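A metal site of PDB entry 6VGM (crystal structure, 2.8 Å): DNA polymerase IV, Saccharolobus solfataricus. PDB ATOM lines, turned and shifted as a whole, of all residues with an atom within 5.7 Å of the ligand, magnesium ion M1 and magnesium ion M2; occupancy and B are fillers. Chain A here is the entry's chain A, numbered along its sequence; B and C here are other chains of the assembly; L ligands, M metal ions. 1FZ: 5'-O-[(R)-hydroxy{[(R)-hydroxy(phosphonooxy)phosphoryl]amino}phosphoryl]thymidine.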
ATOM      1  N   ASP A   7     -13.696 -18.219  23.010  1.00  0.00           N
ATOM      2  CA  ASP A   7     -14.924 -18.112  22.245  1.00  0.00           C
ATOM      3  C   ASP A   7     -15.800 -19.304  22.583  1.00  0.00           C
ATOM      4  O   ASP A   7     -15.364 -20.452  22.463  1.00  0.00           O
ATOM      5  CB  ASP A   7     -14.652 -18.053  20.740  1.00  0.00           C
ATOM      6  CG  ASP A   7     -15.936 -18.101  19.912  1.00  0.00           C
ATOM      7  OD1 ASP A   7     -16.451 -19.207  19.683  1.00  0.00           O
ATOM      8  OD2 ASP A   7     -16.429 -17.023  19.518  1.00  0.00           O
ATOM      9  N   PHE A   8     -17.029 -19.029  23.005  1.00  0.00           N
ATOM     10  CA  PHE A   8     -17.925 -20.076  23.453  1.00  0.00           C
ATOM     11  C   PHE A   8     -18.350 -20.951  22.276  1.00  0.00           C
ATOM     12  O   PHE A   8     -18.380 -20.508  21.126  1.00  0.00           O
ATOM     13  CB  PHE A   8     -19.165 -19.488  24.131  1.00  0.00           C
ATOM     14  CG  PHE A   8     -18.856 -18.394  25.123  1.00  0.00           C
ATOM     15  CD1 PHE A   8     -17.618 -18.318  25.759  1.00  0.00           C
ATOM     16  CD2 PHE A   8     -19.816 -17.437  25.426  1.00  0.00           C
ATOM     17  CE1 PHE A   8     -17.344 -17.307  26.664  1.00  0.00           C
ATOM     18  CE2 PHE A   8     -19.548 -16.429  26.339  1.00  0.00           C
ATOM     19  CZ  PHE A   8     -18.312 -16.359  26.959  1.00  0.00           C
ATOM     20  N   ASP A   9     -18.655 -22.216  22.569  1.00  0.00           N
ATOM     21  CA  ASP A   9     -19.014 -23.179  21.541  1.00  0.00           C
ATOM     22  C   ASP A   9     -20.517 -23.184  21.314  1.00  0.00           C
ATOM     23  O   ASP A   9     -21.287 -23.282  22.282  1.00  0.00           O
ATOM     24  CB  ASP A   9     -18.533 -24.580  21.930  1.00  0.00           C
ATOM     25  CG  ASP A   9     -17.093 -24.585  22.397  1.00  0.00           C
ATOM     26  OD1 ASP A   9     -16.190 -24.364  21.554  1.00  0.00           O
ATOM     27  OD2 ASP A   9     -16.856 -24.817  23.600  1.00  0.00           O
ATOM     28  N   TYR A  10     -20.929 -23.096  20.050  1.00  0.00           N
ATOM     29  CA  TYR A  10     -22.332 -22.967  19.636  1.00  0.00           C
ATOM     30  C   TYR A  10     -23.147 -22.204  20.679  1.00  0.00           C
ATOM     31  O   TYR A  10     -24.123 -22.730  21.214  1.00  0.00           O
ATOM     32  CB  TYR A  10     -22.934 -24.349  19.321  1.00  0.00           C
ATOM     33  CG  TYR A  10     -22.961 -25.349  20.470  1.00  0.00           C
ATOM     34  CD1 TYR A  10     -21.836 -26.077  20.815  1.00  0.00           C
ATOM     35  CD2 TYR A  10     -24.141 -25.594  21.166  1.00  0.00           C
ATOM     36  CE1 TYR A  10     -21.870 -26.995  21.851  1.00  0.00           C
ATOM     37  CE2 TYR A  10     -24.185 -26.502  22.200  1.00  0.00           C
ATOM     38  CZ  TYR A  10     -23.051 -27.205  22.534  1.00  0.00           C
ATOM     39  OH  TYR A  10     -23.102 -28.122  23.560  1.00  0.00           O
ATOM     40  N   PHE A  11     -22.761 -20.954  20.948  1.00  0.00           N
ATOM     41  CA  PHE A  11     -23.136 -20.294  22.198  1.00  0.00           C
ATOM     42  C   PHE A  11     -24.641 -20.294  22.439  1.00  0.00           C
ATOM     43  O   PHE A  11     -25.113 -20.753  23.487  1.00  0.00           O
ATOM     44  CB  PHE A  11     -22.601 -18.853  22.207  1.00  0.00           C
ATOM     45  CG  PHE A  11     -23.024 -18.072  23.418  1.00  0.00           C
ATOM     46  CD1 PHE A  11     -22.791 -18.574  24.689  1.00  0.00           C
ATOM     47  CD2 PHE A  11     -23.677 -16.863  23.287  1.00  0.00           C
ATOM     48  CE1 PHE A  11     -23.187 -17.858  25.809  1.00  0.00           C
ATOM     49  CE2 PHE A  11     -24.069 -16.135  24.401  1.00  0.00           C
ATOM     50  CZ  PHE A  11     -23.831 -16.634  25.664  1.00  0.00           C
ATOM     51  N   TYR A  12     -25.415 -19.772  21.485  1.00  0.00           N
ATOM     52  CA  TYR A  12     -26.846 -19.604  21.705  1.00  0.00           C
ATOM     53  C   TYR A  12     -27.524 -20.930  22.026  1.00  0.00           C
ATOM     54  O   TYR A  12     -28.344 -21.008  22.944  1.00  0.00           O
ATOM     55  CB  TYR A  12     -27.500 -18.972  20.470  1.00  0.00           C
ATOM     56  CG  TYR A  12     -27.302 -17.481  20.344  1.00  0.00           C
ATOM     57  CD1 TYR A  12     -26.375 -16.808  21.131  1.00  0.00           C
ATOM     58  CD2 TYR A  12     -28.042 -16.746  19.421  1.00  0.00           C
ATOM     59  CE1 TYR A  12     -26.196 -15.443  21.000  1.00  0.00           C
ATOM     60  CE2 TYR A  12     -27.856 -15.388  19.279  1.00  0.00           C
ATOM     61  CZ  TYR A  12     -26.938 -14.739  20.077  1.00  0.00           C
ATOM     62  OH  TYR A  12     -26.758 -13.383  19.944  1.00  0.00           O
ATOM     63  N   ALA A  13     -27.177 -21.986  21.289  1.00  0.00           N
ATOM     64  CA  ALA A  13     -27.809 -23.287  21.499  1.00  0.00           C
ATOM     65  C   ALA A  13     -27.435 -23.883  22.852  1.00  0.00           C
ATOM     66  O   ALA A  13     -28.285 -24.432  23.545  1.00  0.00           O
ATOM     67  CB  ALA A  13     -27.424 -24.240  20.366  1.00  0.00           C
ATOM     68  N   VAL A  32     -33.961 -17.014  14.062  1.00  0.00           N
ATOM     69  CA  VAL A  32     -34.474 -15.654  14.069  1.00  0.00           C
ATOM     70  C   VAL A  32     -35.639 -15.639  13.092  1.00  0.00           C
ATOM     71  O   VAL A  32     -35.438 -15.624  11.871  1.00  0.00           O
ATOM     72  CB  VAL A  32     -33.405 -14.634  13.661  1.00  0.00           C
ATOM     73  CG1 VAL A  32     -33.824 -13.214  14.043  1.00  0.00           C
ATOM     74  CG2 VAL A  32     -32.056 -15.009  14.266  1.00  0.00           C
ATOM     75  N   VAL A  43     -30.828 -18.828  10.420  1.00  0.00           N
ATOM     76  CA  VAL A  43     -30.335 -19.638  11.531  1.00  0.00           C
ATOM     77  C   VAL A  43     -29.220 -18.866  12.212  1.00  0.00           C
ATOM     78  O   VAL A  43     -28.205 -18.540  11.586  1.00  0.00           O
ATOM     79  CB  VAL A  43     -29.868 -21.027  11.054  1.00  0.00           C
ATOM     80  CG1 VAL A  43     -29.080 -21.724  12.155  1.00  0.00           C
ATOM     81  CG2 VAL A  43     -31.055 -21.868  10.636  1.00  0.00           C
ATOM     82  N   ALA A  44     -29.411 -18.555  13.499  1.00  0.00           N
ATOM     83  CA  ALA A  44     -28.369 -17.888  14.270  1.00  0.00           C
ATOM     84  C   ALA A  44     -27.204 -18.825  14.521  1.00  0.00           C
ATOM     85  O   ALA A  44     -26.058 -18.535  14.138  1.00  0.00           O
ATOM     86  CB  ALA A  44     -28.954 -17.356  15.578  1.00  0.00           C
ATOM     87  N   THR A  45     -27.467 -19.947  15.172  1.00  0.00           N
ATOM     88  CA  THR A  45     -26.465 -20.983  15.349  1.00  0.00           C
ATOM     89  C   THR A  45     -27.158 -22.320  15.520  1.00  0.00           C
ATOM     90  O   THR A  45     -28.358 -22.391  15.808  1.00  0.00           O
ATOM     91  CB  THR A  45     -25.538 -20.695  16.548  1.00  0.00           C
ATOM     92  OG1 THR A  45     -24.269 -21.329  16.340  1.00  0.00           O
ATOM     93  CG2 THR A  45     -26.158 -21.217  17.850  1.00  0.00           C
ATOM     94  N   ALA A  46     -26.403 -23.393  15.307  1.00  0.00           N
ATOM     95  CA  ALA A  46     -26.865 -24.744  15.559  1.00  0.00           C
ATOM     96  C   ALA A  46     -25.755 -25.514  16.274  1.00  0.00           C
ATOM     97  O   ALA A  46     -24.570 -25.281  16.032  1.00  0.00           O
ATOM     98  CB  ALA A  46     -27.257 -25.470  14.269  1.00  0.00           C
ATOM     99  N   TYR A  48     -23.421 -28.816  17.371  1.00  0.00           N
ATOM    100  CA  TYR A  48     -22.528 -29.550  16.473  1.00  0.00           C
ATOM    101  C   TYR A  48     -23.130 -30.859  15.974  1.00  0.00           C
ATOM    102  O   TYR A  48     -22.709 -31.351  14.920  1.00  0.00           O
ATOM    103  CB  TYR A  48     -21.195 -29.793  17.161  1.00  0.00           C
ATOM    104  CG  TYR A  48     -20.269 -28.608  17.050  1.00  0.00           C
ATOM    105  CD1 TYR A  48     -20.456 -27.486  17.860  1.00  0.00           C
ATOM    106  CD2 TYR A  48     -19.246 -28.582  16.119  1.00  0.00           C
ATOM    107  CE1 TYR A  48     -19.624 -26.394  17.755  1.00  0.00           C
ATOM    108  CE2 TYR A  48     -18.409 -27.488  16.006  1.00  0.00           C
ATOM    109  CZ  TYR A  48     -18.605 -26.390  16.827  1.00  0.00           C
ATOM    110  OH  TYR A  48     -17.772 -25.299  16.723  1.00  0.00           O
ATOM    111  N   ARG A  51     -24.957 -29.206  13.330  1.00  0.00           N
ATOM    112  CA  ARG A  51     -23.958 -28.620  12.437  1.00  0.00           C
ATOM    113  C   ARG A  51     -23.283 -29.688  11.584  1.00  0.00           C
ATOM    114  O   ARG A  51     -22.801 -29.379  10.480  1.00  0.00           O
ATOM    115  CB  ARG A  51     -22.918 -27.838  13.245  1.00  0.00           C
ATOM    116  CG  ARG A  51     -22.160 -26.812  12.421  1.00  0.00           C
ATOM    117  CD  ARG A  51     -21.204 -25.979  13.279  1.00  0.00           C
ATOM    118  NE  ARG A  51     -21.885 -25.329  14.395  1.00  0.00           N
ATOM    119  CZ  ARG A  51     -21.310 -24.454  15.210  1.00  0.00           C
ATOM    120  NH1 ARG A  51     -20.039 -24.117  15.033  1.00  0.00           N
ATOM    121  NH2 ARG A  51     -21.995 -23.906  16.203  1.00  0.00           N
ATOM    122  N   ALA A  57     -24.731 -21.156  10.621  1.00  0.00           N
ATOM    123  CA  ALA A  57     -25.196 -19.778  10.763  1.00  0.00           C
ATOM    124  C   ALA A  57     -25.390 -19.140   9.390  1.00  0.00           C
ATOM    125  O   ALA A  57     -24.581 -19.334   8.472  1.00  0.00           O
ATOM    126  CB  ALA A  57     -24.200 -18.974  11.588  1.00  0.00           C
ATOM    127  N   GLY A  58     -26.470 -18.381   9.244  1.00  0.00           N
ATOM    128  CA  GLY A  58     -26.747 -17.631   8.041  1.00  0.00           C
ATOM    129  C   GLY A  58     -27.633 -18.312   7.031  1.00  0.00           C
ATOM    130  O   GLY A  58     -28.042 -17.677   6.050  1.00  0.00           O
ATOM    131  N   MET A  76     -34.912 -17.241  19.127  1.00  0.00           N
ATOM    132  CA  MET A  76     -33.794 -16.685  19.873  1.00  0.00           C
ATOM    133  C   MET A  76     -34.284 -15.873  21.064  1.00  0.00           C
ATOM    134  O   MET A  76     -35.220 -15.065  20.939  1.00  0.00           O
ATOM    135  CB  MET A  76     -32.931 -15.811  18.953  1.00  0.00           C
ATOM    136  CG  MET A  76     -31.523 -15.617  19.441  1.00  0.00           C
ATOM    137  SD  MET A  76     -30.879 -13.990  19.003  1.00  0.00           S
ATOM    138  CE  MET A  76     -31.614 -13.733  17.407  1.00  0.00           C
ATOM    139  N   SER A 103     -17.219  -9.729  21.249  1.00  0.00           N
ATOM    140  CA  SER A 103     -18.596  -9.929  20.827  1.00  0.00           C
ATOM    141  C   SER A 103     -19.439 -10.554  21.942  1.00  0.00           C
ATOM    142  O   SER A 103     -19.053 -10.513  23.110  1.00  0.00           O
ATOM    143  CB  SER A 103     -18.668 -10.828  19.584  1.00  0.00           C
ATOM    144  OG  SER A 103     -17.894 -12.006  19.753  1.00  0.00           O
ATOM    145  N   ILE A 104     -20.584 -11.122  21.569  1.00  0.00           N
ATOM    146  CA  ILE A 104     -21.453 -11.764  22.550  1.00  0.00           C
ATOM    147  C   ILE A 104     -20.773 -12.974  23.178  1.00  0.00           C
ATOM    148  O   ILE A 104     -21.063 -13.331  24.326  1.00  0.00           O
ATOM    149  CB  ILE A 104     -22.802 -12.148  21.900  1.00  0.00           C
ATOM    150  CG1 ILE A 104     -23.816 -12.603  22.952  1.00  0.00           C
ATOM    151  CG2 ILE A 104     -22.616 -13.248  20.863  1.00  0.00           C
ATOM    152  CD1 ILE A 104     -24.190 -11.528  23.948  1.00  0.00           C
ATOM    153  N   ASP A 105     -19.840 -13.619  22.458  1.00  0.00           N
ATOM    154  CA  ASP A 105     -19.269 -14.884  22.913  1.00  0.00           C
ATOM    155  C   ASP A 105     -17.744 -14.911  22.848  1.00  0.00           C
ATOM    156  O   ASP A 105     -17.155 -15.991  22.908  1.00  0.00           O
ATOM    157  CB  ASP A 105     -19.863 -16.055  22.108  1.00  0.00           C
ATOM    158  CG  ASP A 105     -19.132 -16.311  20.788  1.00  0.00           C
ATOM    159  OD1 ASP A 105     -18.909 -15.354  20.008  1.00  0.00           O
ATOM    160  OD2 ASP A 105     -18.792 -17.476  20.515  1.00  0.00           O
ATOM    161  N   GLU A 106     -17.099 -13.750  22.772  1.00  0.00           N
ATOM    162  CA  GLU A 106     -15.659 -13.712  22.527  1.00  0.00           C
ATOM    163  C   GLU A 106     -14.967 -12.723  23.455  1.00  0.00           C
ATOM    164  O   GLU A 106     -15.501 -11.653  23.746  1.00  0.00           O
ATOM    165  CB  GLU A 106     -15.348 -13.342  21.076  1.00  0.00           C
ATOM    166  CG  GLU A 106     -15.691 -14.433  20.101  1.00  0.00           C
ATOM    167  CD  GLU A 106     -16.065 -13.907  18.737  1.00  0.00           C
ATOM    168  OE1 GLU A 106     -15.142 -13.552  17.976  1.00  0.00           O
ATOM    169  OE2 GLU A 106     -17.271 -13.855  18.434  1.00  0.00           O
ATOM    170  N   LYS A 159     -12.070 -25.937  18.211  1.00  0.00           N
ATOM    171  CA  LYS A 159     -13.496 -26.083  18.514  1.00  0.00           C
ATOM    172  C   LYS A 159     -13.971 -27.495  18.160  1.00  0.00           C
ATOM    173  O   LYS A 159     -13.632 -27.999  17.086  1.00  0.00           O
ATOM    174  CB  LYS A 159     -14.325 -25.039  17.761  1.00  0.00           C
ATOM    175  CG  LYS A 159     -13.766 -23.641  17.820  1.00  0.00           C
ATOM    176  CD  LYS A 159     -14.871 -22.600  17.851  1.00  0.00           C
ATOM    177  CE  LYS A 159     -15.555 -22.568  19.199  1.00  0.00           C
ATOM    178  NZ  LYS A 159     -15.161 -21.449  20.093  1.00  0.00           N
ATOM    179  N   PRO A 160     -14.781 -28.145  19.003  1.00  0.00           N
ATOM    180  CA  PRO A 160     -15.299 -27.619  20.278  1.00  0.00           C
ATOM    181  C   PRO A 160     -14.593 -28.154  21.518  1.00  0.00           C
ATOM    182  O   PRO A 160     -13.731 -29.023  21.390  1.00  0.00           O
ATOM    183  CB  PRO A 160     -16.755 -28.084  20.259  1.00  0.00           C
ATOM    184  CG  PRO A 160     -16.694 -29.408  19.535  1.00  0.00           C
ATOM    185  CD  PRO A 160     -15.467 -29.393  18.632  1.00  0.00           C
ATOM    186  P   A38 B   5     -36.198 -12.893   6.488  1.00  0.00           P
ATOM    187  O1P A38 B   5     -37.282 -13.854   6.231  1.00  0.00           O
ATOM    188  O2P A38 B   5     -35.969 -11.766   5.546  1.00  0.00           O
ATOM    189  O5' A38 B   5     -35.250 -13.048   7.786  1.00  0.00           O
ATOM    190  C5' A38 B   5     -34.674 -11.874   8.309  1.00  0.00           C
ATOM    191  C4' A38 B   5     -34.519 -12.060   9.809  1.00  0.00           C
ATOM    192  O4' A38 B   5     -33.377 -13.091  10.087  1.00  0.00           O
ATOM    193  C3' A38 B   5     -34.131 -10.942  10.366  1.00  0.00           C
ATOM    194  O3' A38 B   5     -34.634 -10.887  11.727  1.00  0.00           O
ATOM    195  C2' A38 B   5     -32.511 -11.011  10.409  1.00  0.00           C
ATOM    196  C1' A38 B   5     -32.273 -12.255  10.758  1.00  0.00           C
ATOM    197  N9  A38 B   5     -30.943 -12.688  10.262  1.00  0.00           N
ATOM    198  C8  A38 B   5     -30.527 -12.803   8.901  1.00  0.00           C
ATOM    199  N7  A38 B   5     -29.158 -13.257   8.901  1.00  0.00           N
ATOM    200  C5  A38 B   5     -28.721 -13.404  10.309  1.00  0.00           C
ATOM    201  C6  A38 B   5     -27.523 -13.801  10.946  1.00  0.00           C
ATOM    202  N6  A38 B   5     -26.375 -14.159  10.163  1.00  0.00           N
ATOM    203  N1  A38 B   5     -27.496 -13.815  12.274  1.00  0.00           N
ATOM    204  C2  A38 B   5     -28.541 -13.485  13.040  1.00  0.00           C
ATOM    205  N3  A38 B   5     -29.686 -13.111  12.465  1.00  0.00           N
ATOM    206  C4  A38 B   5     -29.800 -13.061  11.131  1.00  0.00           C
ATOM    207  O   A38 B   5     -31.189 -12.585   7.952  1.00  0.00           O
ATOM    208  P    DG B   6     -35.406  -9.534  11.715  1.00  0.00           P
ATOM    209  OP1  DG B   6     -36.506  -9.861  12.656  1.00  0.00           O
ATOM    210  OP2  DG B   6     -35.644  -8.654  10.543  1.00  0.00           O
ATOM    211  O5'  DG B   6     -34.178  -8.952  12.552  1.00  0.00           O
ATOM    212  C5'  DG B   6     -33.793  -9.571  13.769  1.00  0.00           C
ATOM    213  C4'  DG B   6     -32.381  -9.203  14.158  1.00  0.00           C
ATOM    214  O4'  DG B   6     -31.428  -9.806  13.256  1.00  0.00           O
ATOM    215  C3'  DG B   6     -32.051  -7.701  14.144  1.00  0.00           C
ATOM    216  O3'  DG B   6     -31.881  -7.261  15.493  1.00  0.00           O
ATOM    217  C2'  DG B   6     -30.726  -7.602  13.343  1.00  0.00           C
ATOM    218  C1'  DG B   6     -30.250  -9.057  13.366  1.00  0.00           C
ATOM    219  N9   DG B   6     -29.333  -9.425  12.286  1.00  0.00           N
ATOM    220  C8   DG B   6     -29.579  -9.402  10.933  1.00  0.00           C
ATOM    221  N7   DG B   6     -28.565  -9.809  10.208  1.00  0.00           N
ATOM    222  C5   DG B   6     -27.585 -10.120  11.142  1.00  0.00           C
ATOM    223  C6   DG B   6     -26.273 -10.612  10.959  1.00  0.00           C
ATOM    224  O6   DG B   6     -25.697 -10.878   9.894  1.00  0.00           O
ATOM    225  N1   DG B   6     -25.612 -10.787  12.167  1.00  0.00           N
ATOM    226  C2   DG B   6     -26.155 -10.535  13.408  1.00  0.00           C
ATOM    227  N2   DG B   6     -25.367 -10.770  14.456  1.00  0.00           N
ATOM    228  N3   DG B   6     -27.389 -10.079  13.592  1.00  0.00           N
ATOM    229  C4   DG B   6     -28.045  -9.891  12.416  1.00  0.00           C
ATOM    230  P    DC C  13     -16.079 -14.275  13.600  1.00  0.00           P
ATOM    231  OP1  DC C  13     -14.865 -14.880  14.203  1.00  0.00           O
ATOM    232  OP2  DC C  13     -16.771 -14.951  12.482  1.00  0.00           O
ATOM    233  O5'  DC C  13     -17.195 -14.065  14.735  1.00  0.00           O
ATOM    234  C5'  DC C  13     -17.214 -12.887  15.547  1.00  0.00           C
ATOM    235  C4'  DC C  13     -18.629 -12.627  16.043  1.00  0.00           C
ATOM    236  O4'  DC C  13     -19.449 -12.057  14.977  1.00  0.00           O
ATOM    237  C3'  DC C  13     -19.372 -13.878  16.519  1.00  0.00           C
ATOM    238  O3'  DC C  13     -20.054 -13.602  17.742  1.00  0.00           O
ATOM    239  C2'  DC C  13     -20.361 -14.138  15.389  1.00  0.00           C
ATOM    240  C1'  DC C  13     -20.694 -12.721  14.988  1.00  0.00           C
ATOM    241  N1   DC C  13     -21.350 -12.632  13.644  1.00  0.00           N
ATOM    242  C2   DC C  13     -22.620 -12.056  13.537  1.00  0.00           C
ATOM    243  O2   DC C  13     -23.161 -11.605  14.551  1.00  0.00           O
ATOM    244  N3   DC C  13     -23.210 -11.984  12.315  1.00  0.00           N
ATOM    245  C4   DC C  13     -22.594 -12.477  11.249  1.00  0.00           C
ATOM    246  N4   DC C  13     -23.221 -12.389  10.070  1.00  0.00           N
ATOM    247  C5   DC C  13     -21.302 -13.077  11.337  1.00  0.00           C
ATOM    248  C6   DC C  13     -20.724 -13.144  12.541  1.00  0.00           C
HETATM  249  O2  1FZ L   1     -26.509 -14.651  15.275  1.00  0.00           O
HETATM  250  O4  1FZ L   1     -24.058 -15.336  11.518  1.00  0.00           O
HETATM  251  C4  1FZ L   1     -24.152 -15.417  12.747  1.00  0.00           C
HETATM  252  C5  1FZ L   1     -23.127 -15.920  13.522  1.00  0.00           C
HETATM  253  C6  1FZ L   1     -23.295 -15.985  14.895  1.00  0.00           C
HETATM  254  C5M 1FZ L   1     -21.956 -16.369  12.920  1.00  0.00           C
HETATM  255  N3  1FZ L   1     -25.307 -14.986  13.378  1.00  0.00           N
HETATM  256  C2  1FZ L   1     -25.458 -15.052  14.761  1.00  0.00           C
HETATM  257  N1  1FZ L   1     -24.479 -15.538  15.537  1.00  0.00           N
HETATM  258  C1' 1FZ L   1     -24.719 -15.580  17.031  1.00  0.00           C
HETATM  259  C2' 1FZ L   1     -25.146 -16.946  17.571  1.00  0.00           C
HETATM  260  C3' 1FZ L   1     -23.791 -17.604  17.740  1.00  0.00           C
HETATM  261  O3' 1FZ L   1     -23.855 -18.742  18.660  1.00  0.00           O
HETATM  262  O4' 1FZ L   1     -23.642 -15.259  17.967  1.00  0.00           O
HETATM  263  C4' 1FZ L   1     -22.949 -16.480  18.341  1.00  0.00           C
HETATM  264  C5' 1FZ L   1     -21.626 -16.387  17.599  1.00  0.00           C
HETATM  265  O5' 1FZ L   1     -20.623 -17.259  18.089  1.00  0.00           O
HETATM  266  PA  1FZ L   1     -19.674 -17.964  17.027  1.00  0.00           P
HETATM  267  O1A 1FZ L   1     -18.270 -18.128  17.492  1.00  0.00           O
HETATM  268  O2A 1FZ L   1     -19.725 -17.106  15.659  1.00  0.00           O
HETATM  269  N3A 1FZ L   1     -20.436 -19.345  16.587  1.00  0.00           N
HETATM  270  PB  1FZ L   1     -20.930 -20.265  17.861  1.00  0.00           P
HETATM  271  O1B 1FZ L   1     -22.527 -20.420  17.807  1.00  0.00           O
HETATM  272  O2B 1FZ L   1     -20.448 -19.895  19.224  1.00  0.00           O
HETATM  273  O3B 1FZ L   1     -20.393 -21.679  17.420  1.00  0.00           O
HETATM  274  PG  1FZ L   1     -18.828 -21.972  17.427  1.00  0.00           P
HETATM  275  O1G 1FZ L   1     -18.044 -20.722  18.083  1.00  0.00           O
HETATM  276  O3G 1FZ L   1     -18.555 -23.236  18.160  1.00  0.00           O
HETATM  277  O2G 1FZ L   1     -18.340 -21.998  15.882  1.00  0.00           O
HETATM  278 MG    MG M   1     -18.624 -19.295  19.545  1.00  0.00          MG
HETATM  279 MG    MG M   2     -17.402 -16.121  17.704  1.00  0.00          MG
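O1A of the ligand is bound to magnesium ion M2, at 2.2 Å. Magnesium ion M2 is bound by OD2 of Asp 7 (2.2 Å). OE2 of Glu 106 is bound to magnesium ion M2.
Merely in contact with magnesium ion M2: DC 13 of chain C. Of the 26 residues printed, 4 come within 4 Å of magnesium ion M2. The nearest printed residue that does not touch magnesium ion M2 is Ser 103 (4.6 Å).
Magnesium ion M1 is bound by O2B of the ligand (1.9 Å), O of Phe 8 (2.0 Å), OD2 of Asp 105 (2.1 Å), O1G of the ligand (2.1 Å), OD1 of Asp 7 (2.2 Å) and O1A of the ligand (2.4 Å).
Three residues have an atom within 4 Å of magnesium ion M1: Asp 7, Phe 8 and Asp 105. The nearest printed residue that does not touch magnesium ion M1 is Lys 159 (4.1 Å).
N4 of DC 13 of chain C lies close to an oxygen (O4) of the ligand, 3.4 Å away. Asp 9 touches the ligand (CA to O3G, 3.4 Å). Ala 44 touches the ligand (O to C2, 3.6 Å). Ala 57 touches the ligand (CB to O4, 3.6 Å). Ile 104 touches the ligand (CG2 to O4', 3.7 Å). Within 4 Å of the ligand: Asp 7, Phe 8, Asp 9, Tyr 10, Phe 11, Tyr 12, Ala 44, Thr 45, Tyr 48, Arg 51, Ala 57, Ile 104, Asp 105, Lys 159, A38 5 of chain B and DC 13 of chain C.
An oxygen (O1B) of the ligand lies within hydrogen-bond range of the side-chain hydroxyl of Thr 45 (2.5 Å). The side-chain hydroxyl of Tyr 48 sits at hydrogen-bond distance from an oxygen (O3G) of the ligand. A nitrogen (N3) of the ligand lies within hydrogen-bond range of N1 of A38 5 of chain B (2.7 Å). An oxygen (O2G) of the ligand lies within salt-bridge range of the guanidinium group (NH1) of Arg 51 (2.8 Å). N of Tyr 10 lies within hydrogen-bond range of O3B of the ligand, at 3.0 Å. The backbone NH of Phe 11 lies within hydrogen-bond range of an oxygen (O1B) of the ligand, 3.2 Å away. An oxygen (O1G) of the ligand lies close to the side-chain amino group of Lys 159 (3.6 Å). An oxygen (O3') of the ligand sits at hydrogen-bond distance from the backbone NH of Tyr 12 (3.4 Å).
OD1 of Asp 105 sits close to OE2 of Glu 106 (2.7 Å). The backbone carbonyl oxygen (O) of Asp 7 sits at hydrogen-bond distance from the side-chain amino group (NZ) of Lys 159, at 2.6 Å. OG1 of Thr 45 lies within hydrogen-bond range of NH2 of Arg 51, at 3.4 Å. OH of Tyr 48 sits at hydrogen-bond distance from NH1 of Arg 51 (3.1 Å). The backbone carbonyl oxygen (O) of Ala 46 sits at hydrogen-bond distance from the guanidinium group (NH2) of Arg 51, at 2.9 Å. N3 of DC 13 of chain C lies close to N1 of DG 6 of chain B (2.7 Å). O3' of DC 13 of chain C is in hydrogen-bond range of OG of Ser 103, 3.4 Å away. The side-chain amino group (NZ) of Lys 159 is in salt-bridge range of the side-chain carboxylate (OD1) of Asp 9 (3.4 Å).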
